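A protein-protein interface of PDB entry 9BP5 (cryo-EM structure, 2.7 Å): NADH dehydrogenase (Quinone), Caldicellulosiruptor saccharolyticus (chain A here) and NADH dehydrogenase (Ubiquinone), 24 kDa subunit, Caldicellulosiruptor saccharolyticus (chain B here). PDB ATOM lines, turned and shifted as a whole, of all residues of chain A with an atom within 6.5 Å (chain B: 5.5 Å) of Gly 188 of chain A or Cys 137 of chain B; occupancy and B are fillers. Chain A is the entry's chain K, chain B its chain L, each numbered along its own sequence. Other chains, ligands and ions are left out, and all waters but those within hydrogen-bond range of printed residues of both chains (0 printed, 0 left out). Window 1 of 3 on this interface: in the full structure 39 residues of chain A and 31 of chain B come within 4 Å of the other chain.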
ATOM      1  N   SER A   9     -17.980  29.358 -21.339  1.00  0.00           N
ATOM      2  CA  SER A   9     -16.771  28.856 -20.697  1.00  0.00           C
ATOM      3  C   SER A   9     -15.717  29.953 -20.621  1.00  0.00           C
ATOM      4  O   SER A   9     -15.026  30.094 -19.607  1.00  0.00           O
ATOM      5  CB  SER A   9     -16.239  27.639 -21.453  1.00  0.00           C
ATOM      6  OG  SER A   9     -15.026  27.171 -20.887  1.00  0.00           O
ATOM      7  N   GLU A 184     -15.582  16.729 -26.286  1.00  0.00           N
ATOM      8  CA  GLU A 184     -14.652  17.496 -27.110  1.00  0.00           C
ATOM      9  C   GLU A 184     -13.252  16.961 -26.821  1.00  0.00           C
ATOM     10  O   GLU A 184     -12.538  17.474 -25.958  1.00  0.00           O
ATOM     11  CB  GLU A 184     -14.763  18.989 -26.825  1.00  0.00           C
ATOM     12  CG  GLU A 184     -14.209  19.890 -27.919  1.00  0.00           C
ATOM     13  CD  GLU A 184     -14.625  19.471 -29.319  1.00  0.00           C
ATOM     14  OE1 GLU A 184     -13.983  18.570 -29.901  1.00  0.00           O
ATOM     15  OE2 GLU A 184     -15.597  20.054 -29.843  1.00  0.00           O
ATOM     16  N   GLY A 185     -12.868  15.914 -27.554  1.00  0.00           N
ATOM     17  CA  GLY A 185     -11.608  15.246 -27.273  1.00  0.00           C
ATOM     18  C   GLY A 185     -10.390  16.097 -27.574  1.00  0.00           C
ATOM     19  O   GLY A 185      -9.384  16.026 -26.865  1.00  0.00           O
ATOM     20  N   ASP A 186     -10.460  16.904 -28.625  1.00  0.00           N
ATOM     21  CA  ASP A 186      -9.313  17.682 -29.072  1.00  0.00           C
ATOM     22  C   ASP A 186      -8.899  18.682 -27.998  1.00  0.00           C
ATOM     23  O   ASP A 186      -9.717  19.524 -27.597  1.00  0.00           O
ATOM     24  CB  ASP A 186      -9.660  18.400 -30.375  1.00  0.00           C
ATOM     25  CG  ASP A 186      -8.572  19.348 -30.837  1.00  0.00           C
ATOM     26  OD1 ASP A 186      -7.393  19.132 -30.497  1.00  0.00           O
ATOM     27  OD2 ASP A 186      -8.897  20.312 -31.557  1.00  0.00           O
ATOM     28  N   PRO A 187      -7.662  18.629 -27.507  1.00  0.00           N
ATOM     29  CA  PRO A 187      -7.221  19.596 -26.495  1.00  0.00           C
ATOM     30  C   PRO A 187      -6.905  20.955 -27.096  1.00  0.00           C
ATOM     31  O   PRO A 187      -5.744  21.259 -27.389  1.00  0.00           O
ATOM     32  CB  PRO A 187      -5.970  18.935 -25.908  1.00  0.00           C
ATOM     33  CG  PRO A 187      -5.442  18.111 -27.020  1.00  0.00           C
ATOM     34  CD  PRO A 187      -6.636  17.610 -27.780  1.00  0.00           C
ATOM     35  N   GLY A 188      -7.928  21.781 -27.283  1.00  0.00           N
ATOM     36  CA  GLY A 188      -7.756  23.052 -27.955  1.00  0.00           C
ATOM     37  C   GLY A 188      -8.971  23.410 -28.782  1.00  0.00           C
ATOM     38  O   GLY A 188      -9.002  24.444 -29.453  1.00  0.00           O
ATOM     39  N   ALA A 189      -9.975  22.543 -28.740  1.00  0.00           N
ATOM     40  CA  ALA A 189     -11.246  22.761 -29.409  1.00  0.00           C
ATOM     41  C   ALA A 189     -12.310  23.079 -28.372  1.00  0.00           C
ATOM     42  O   ALA A 189     -12.358  22.457 -27.308  1.00  0.00           O
ATOM     43  CB  ALA A 189     -11.657  21.532 -30.219  1.00  0.00           C
ATOM     44  N   PHE A 190     -13.158  24.065 -28.678  1.00  0.00           N
ATOM     45  CA  PHE A 190     -14.225  24.431 -27.757  1.00  0.00           C
ATOM     46  C   PHE A 190     -15.536  24.748 -28.471  1.00  0.00           C
ATOM     47  O   PHE A 190     -16.368  25.474 -27.914  1.00  0.00           O
ATOM     48  CB  PHE A 190     -13.808  25.624 -26.896  1.00  0.00           C
ATOM     49  CG  PHE A 190     -13.157  26.732 -27.668  1.00  0.00           C
ATOM     50  CD1 PHE A 190     -13.919  27.728 -28.250  1.00  0.00           C
ATOM     51  CD2 PHE A 190     -11.783  26.785 -27.803  1.00  0.00           C
ATOM     52  CE1 PHE A 190     -13.322  28.747 -28.956  1.00  0.00           C
ATOM     53  CE2 PHE A 190     -11.183  27.803 -28.507  1.00  0.00           C
ATOM     54  CZ  PHE A 190     -11.953  28.786 -29.082  1.00  0.00           C
ATOM     55  N   MET A 191     -15.743  24.238 -29.687  1.00  0.00           N
ATOM     56  CA  MET A 191     -16.993  24.512 -30.388  1.00  0.00           C
ATOM     57  C   MET A 191     -18.173  23.858 -29.679  1.00  0.00           C
ATOM     58  O   MET A 191     -19.217  24.489 -29.479  1.00  0.00           O
ATOM     59  CB  MET A 191     -16.914  24.029 -31.837  1.00  0.00           C
ATOM     60  CG  MET A 191     -16.282  22.661 -32.008  1.00  0.00           C
ATOM     61  SD  MET A 191     -14.493  22.683 -31.895  1.00  0.00           S
ATOM     62  CE  MET A 191     -14.124  23.963 -33.083  1.00  0.00           C
ATOM     63  N   ARG A 193     -18.484  22.883 -26.537  1.00  0.00           N
ATOM     64  CA  ARG A 193     -18.747  23.516 -25.249  1.00  0.00           C
ATOM     65  C   ARG A 193     -19.528  24.808 -25.426  1.00  0.00           C
ATOM     66  O   ARG A 193     -20.509  25.058 -24.717  1.00  0.00           O
ATOM     67  CB  ARG A 193     -17.431  23.785 -24.525  1.00  0.00           C
ATOM     68  CG  ARG A 193     -17.344  23.183 -23.143  1.00  0.00           C
ATOM     69  CD  ARG A 193     -15.986  23.457 -22.530  1.00  0.00           C
ATOM     70  NE  ARG A 193     -14.907  22.974 -23.379  1.00  0.00           N
ATOM     71  CZ  ARG A 193     -13.640  22.893 -23.002  1.00  0.00           C
ATOM     72  NH1 ARG A 193     -13.257  23.249 -21.787  1.00  0.00           N
ATOM     73  NH2 ARG A 193     -12.734  22.439 -23.863  1.00  0.00           N
ATOM     74  N   TYR A 227     -16.904  19.860 -17.794  1.00  0.00           N
ATOM     75  CA  TYR A 227     -17.576  21.083 -18.226  1.00  0.00           C
ATOM     76  C   TYR A 227     -18.848  21.249 -17.410  1.00  0.00           C
ATOM     77  O   TYR A 227     -19.927  20.822 -17.841  1.00  0.00           O
ATOM     78  CB  TYR A 227     -17.897  21.037 -19.722  1.00  0.00           C
ATOM     79  CG  TYR A 227     -16.820  20.419 -20.584  1.00  0.00           C
ATOM     80  CD1 TYR A 227     -15.477  20.673 -20.347  1.00  0.00           C
ATOM     81  CD2 TYR A 227     -17.149  19.588 -21.643  1.00  0.00           C
ATOM     82  CE1 TYR A 227     -14.496  20.111 -21.133  1.00  0.00           C
ATOM     83  CE2 TYR A 227     -16.173  19.023 -22.435  1.00  0.00           C
ATOM     84  CZ  TYR A 227     -14.848  19.287 -22.175  1.00  0.00           C
ATOM     85  OH  TYR A 227     -13.868  18.727 -22.960  1.00  0.00           O
ATOM     86  N   ALA A 342     -12.629  26.703 -34.110  1.00  0.00           N
ATOM     87  CA  ALA A 342     -12.100  27.380 -32.932  1.00  0.00           C
ATOM     88  C   ALA A 342     -10.726  27.907 -33.315  1.00  0.00           C
ATOM     89  O   ALA A 342      -9.752  27.152 -33.351  1.00  0.00           O
ATOM     90  CB  ALA A 342     -12.028  26.440 -31.737  1.00  0.00           C
ATOM     91  N   ALA A 344      -7.411  29.616 -32.661  1.00  0.00           N
ATOM     92  CA  ALA A 344      -6.569  29.863 -31.503  1.00  0.00           C
ATOM     93  C   ALA A 344      -5.112  29.840 -31.942  1.00  0.00           C
ATOM     94  O   ALA A 344      -4.796  29.618 -33.114  1.00  0.00           O
ATOM     95  CB  ALA A 344      -6.844  28.838 -30.403  1.00  0.00           C
ATOM     96  N   GLY A 416     -10.808  22.605 -34.542  1.00  0.00           N
ATOM     97  CA  GLY A 416      -9.762  23.398 -33.928  1.00  0.00           C
ATOM     98  C   GLY A 416      -8.717  23.841 -34.928  1.00  0.00           C
ATOM     99  O   GLY A 416      -8.091  23.004 -35.584  1.00  0.00           O
ATOM    100  N   MET A 417      -8.516  25.151 -35.065  1.00  0.00           N
ATOM    101  CA  MET A 417      -7.531  25.708 -35.983  1.00  0.00           C
ATOM    102  C   MET A 417      -6.494  26.455 -35.159  1.00  0.00           C
ATOM    103  O   MET A 417      -6.785  27.527 -34.615  1.00  0.00           O
ATOM    104  CB  MET A 417      -8.186  26.638 -36.999  1.00  0.00           C
ATOM    105  CG  MET A 417      -7.742  26.395 -38.418  1.00  0.00           C
ATOM    106  SD  MET A 417      -8.212  27.701 -39.560  1.00  0.00           S
ATOM    107  CE  MET A 417      -9.827  28.114 -38.932  1.00  0.00           C
ATOM    108  N   ILE A 418      -5.285  25.907 -35.079  1.00  0.00           N
ATOM    109  CA  ILE A 418      -4.220  26.489 -34.268  1.00  0.00           C
ATOM    110  C   ILE A 418      -3.192  27.117 -35.197  1.00  0.00           C
ATOM    111  O   ILE A 418      -2.532  26.415 -35.967  1.00  0.00           O
ATOM    112  CB  ILE A 418      -3.568  25.445 -33.353  1.00  0.00           C
ATOM    113  CG1 ILE A 418      -4.640  24.604 -32.666  1.00  0.00           C
ATOM    114  CG2 ILE A 418      -2.695  26.121 -32.324  1.00  0.00           C
ATOM    115  CD1 ILE A 418      -5.469  25.373 -31.674  1.00  0.00           C
ATOM    116  N   CYS B  96      -3.739  24.328 -17.685  1.00  0.00           N
ATOM    117  CA  CYS B  96      -4.168  23.969 -19.028  1.00  0.00           C
ATOM    118  C   CYS B  96      -2.963  23.724 -19.922  1.00  0.00           C
ATOM    119  O   CYS B  96      -1.998  24.491 -19.909  1.00  0.00           O
ATOM    120  CB  CYS B  96      -5.046  25.071 -19.615  1.00  0.00           C
ATOM    121  SG  CYS B  96      -5.568  24.766 -21.311  1.00  0.00           S
ATOM    122  N   GLY B  98      -3.558  22.676 -23.395  1.00  0.00           N
ATOM    123  CA  GLY B  98      -4.104  22.524 -24.722  1.00  0.00           C
ATOM    124  C   GLY B  98      -3.145  23.063 -25.761  1.00  0.00           C
ATOM    125  O   GLY B  98      -2.073  23.591 -25.461  1.00  0.00           O
ATOM    126  N   THR B  99      -3.540  22.911 -27.025  1.00  0.00           N
ATOM    127  CA  THR B  99      -2.674  23.345 -28.114  1.00  0.00           C
ATOM    128  C   THR B  99      -2.451  24.851 -28.083  1.00  0.00           C
ATOM    129  O   THR B  99      -1.323  25.322 -28.272  1.00  0.00           O
ATOM    130  CB  THR B  99      -3.263  22.921 -29.456  1.00  0.00           C
ATOM    131  OG1 THR B  99      -3.828  21.612 -29.336  1.00  0.00           O
ATOM    132  CG2 THR B  99      -2.180  22.900 -30.518  1.00  0.00           C
ATOM    133  N   ALA B 100      -3.512  25.622 -27.839  1.00  0.00           N
ATOM    134  CA  ALA B 100      -3.392  27.075 -27.853  1.00  0.00           C
ATOM    135  C   ALA B 100      -2.472  27.566 -26.744  1.00  0.00           C
ATOM    136  O   ALA B 100      -1.618  28.431 -26.967  1.00  0.00           O
ATOM    137  CB  ALA B 100      -4.771  27.712 -27.723  1.00  0.00           C
ATOM    138  N   VAL B 135      -4.478  19.686 -17.661  1.00  0.00           N
ATOM    139  CA  VAL B 135      -5.825  19.494 -18.172  1.00  0.00           C
ATOM    140  C   VAL B 135      -5.862  19.930 -19.629  1.00  0.00           C
ATOM    141  O   VAL B 135      -4.921  20.527 -20.149  1.00  0.00           O
ATOM    142  CB  VAL B 135      -6.878  20.264 -17.349  1.00  0.00           C
ATOM    143  CG1 VAL B 135      -7.191  19.523 -16.062  1.00  0.00           C
ATOM    144  CG2 VAL B 135      -6.388  21.664 -17.051  1.00  0.00           C
ATOM    145  N   ALA B 136      -6.971  19.613 -20.289  1.00  0.00           N
ATOM    146  CA  ALA B 136      -7.191  20.027 -21.666  1.00  0.00           C
ATOM    147  C   ALA B 136      -7.658  21.480 -21.680  1.00  0.00           C
ATOM    148  O   ALA B 136      -7.565  22.196 -20.681  1.00  0.00           O
ATOM    149  CB  ALA B 136      -8.183  19.093 -22.351  1.00  0.00           C
ATOM    150  N   CYS B 137      -8.162  21.933 -22.826  1.00  0.00           N
ATOM    151  CA  CYS B 137      -8.595  23.317 -22.960  1.00  0.00           C
ATOM    152  C   CYS B 137      -9.678  23.647 -21.944  1.00  0.00           C
ATOM    153  O   CYS B 137     -10.628  22.882 -21.758  1.00  0.00           O
ATOM    154  CB  CYS B 137      -9.109  23.573 -24.375  1.00  0.00           C
ATOM    155  SG  CYS B 137      -9.525  25.294 -24.695  1.00  0.00           S
ATOM    156  N   LEU B 138      -9.526  24.790 -21.283  1.00  0.00           N
ATOM    157  CA  LEU B 138     -10.492  25.257 -20.301  1.00  0.00           C
ATOM    158  C   LEU B 138     -11.547  26.174 -20.901  1.00  0.00           C
ATOM    159  O   LEU B 138     -12.402  26.675 -20.166  1.00  0.00           O
ATOM    160  CB  LEU B 138      -9.774  25.973 -19.156  1.00  0.00           C
ATOM    161  CG  LEU B 138      -8.943  25.078 -18.236  1.00  0.00           C
ATOM    162  CD1 LEU B 138      -7.947  25.902 -17.451  1.00  0.00           C
ATOM    163  CD2 LEU B 138      -9.839  24.296 -17.299  1.00  0.00           C
ATOM    164  N   GLY B 139     -11.510  26.404 -22.214  1.00  0.00           N
ATOM    165  CA  GLY B 139     -12.471  27.224 -22.904  1.00  0.00           C
ATOM    166  C   GLY B 139     -12.021  28.654 -23.124  1.00  0.00           C
ATOM    167  O   GLY B 139     -12.440  29.282 -24.103  1.00  0.00           O
ATOM    168  N   CYS B 140     -11.176  29.178 -22.244  1.00  0.00           N
ATOM    169  CA  CYS B 140     -10.678  30.545 -22.364  1.00  0.00           C
ATOM    170  C   CYS B 140      -9.313  30.534 -23.049  1.00  0.00           C
ATOM    171  O   CYS B 140      -8.270  30.778 -22.444  1.00  0.00           O
ATOM    172  CB  CYS B 140     -10.616  31.204 -20.992  1.00  0.00           C
ATOM    173  SG  CYS B 140      -9.970  30.136 -19.693  1.00  0.00           S
ATOM    174  N   CYS B 141      -9.343  30.238 -24.349  1.00  0.00           N
ATOM    175  CA  CYS B 141      -8.107  30.174 -25.119  1.00  0.00           C
ATOM    176  C   CYS B 141      -7.472  31.546 -25.286  1.00  0.00           C
ATOM    177  O   CYS B 141      -6.245  31.647 -25.397  1.00  0.00           O
ATOM    178  CB  CYS B 141      -8.373  29.552 -26.488  1.00  0.00           C
ATOM    179  SG  CYS B 141      -8.171  27.768 -26.551  1.00  0.00           S
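The side-chain hydroxyl (OG) of Ser 9 of chain A is in hydrogen-bond range of the backbone carbonyl oxygen (O) of Leu 138 of chain B (2.8 Å).
The backbone carbonyl oxygen (O) of Pro 187 of chain A sits at hydrogen-bond distance from the side-chain hydroxyl (OG1) of Thr 99 of chain B (2.8 Å).
O of Cys 137 of chain B is in hydrogen-bond range of NH1 of Arg 193 of chain A, 2.7 Å away.
O of Ala 189 of chain A is in hydrogen-bond range of NH2 of Arg 193 of chain A (3.5 Å).
N of Ala 344 of chain A lies within hydrogen-bond range of O of Met 417 of chain A, at 2.9 Å.
The backbone NH (N) of Gly 98 of chain B sits close to the side-chain sulfur (SG) of Cys 96 of chain B.
The backbone NH of Gly 139 of chain B lies close to the side-chain sulfur of Cys 137 of chain B.
Gly 139 of chain B touches Ser 9 of chain A.
Pro 187 of chain A touches Gly 98 of chain B.
Cys 137 of chain B touches Gly 188 of chain A.
Phe 190 of chain A touches Cys 141 of chain B.
Leu 138 of chain B touches Arg 193 of chain A.
Gly 139 of chain B touches Arg 193 of chain A.
Ala 344 of chain A touches Ala 100 of chain B (CB to CB, 3.6 Å).
Ile 418 of chain A touches Thr 99 of chain B.
Of the printed residues of chain B, Ser 9 of chain A touches Leu 138 (2.8 Å) and Gly 139 (3.3 Å).
Printed residues of chain B within 4 Å of Pro 187 of chain A: Gly 98 (3.4 Å) and Thr 99 (2.8 Å).
Of the printed residues of chain B, Gly 188 of chain A touches Cys 137.
Ala 342 of chain A touches none of the printed residues of chain B.
Cys 137 of chain B touches just these residues of chain A: Gly 188 (3.6 Å) and Arg 193 (2.7 Å).
Of the printed residues of chain A, Leu 138 of chain B touches Ser 9 (2.8 Å) and Arg 193 (3.5 Å).
The nearest residue of chain A that does not touch Cys 137 of chain B is Phe 190 of chain A (4.1 Å).
The nearest printed residue of chain B that does not touch Arg 193 of chain A is Ala 136 of chain B (5.6 Å).
Hydrophobic or aromatic side chains of chain B within 4 Å of the printed part of chain A: Ala 100.
Of the 16 printed residues of chain A, 7 touch a printed residue of chain B.
Among the printed residues, no Asp or Glu carboxylate lies within 4 Å of a Lys or Arg side-chain nitrogen of the other chain.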
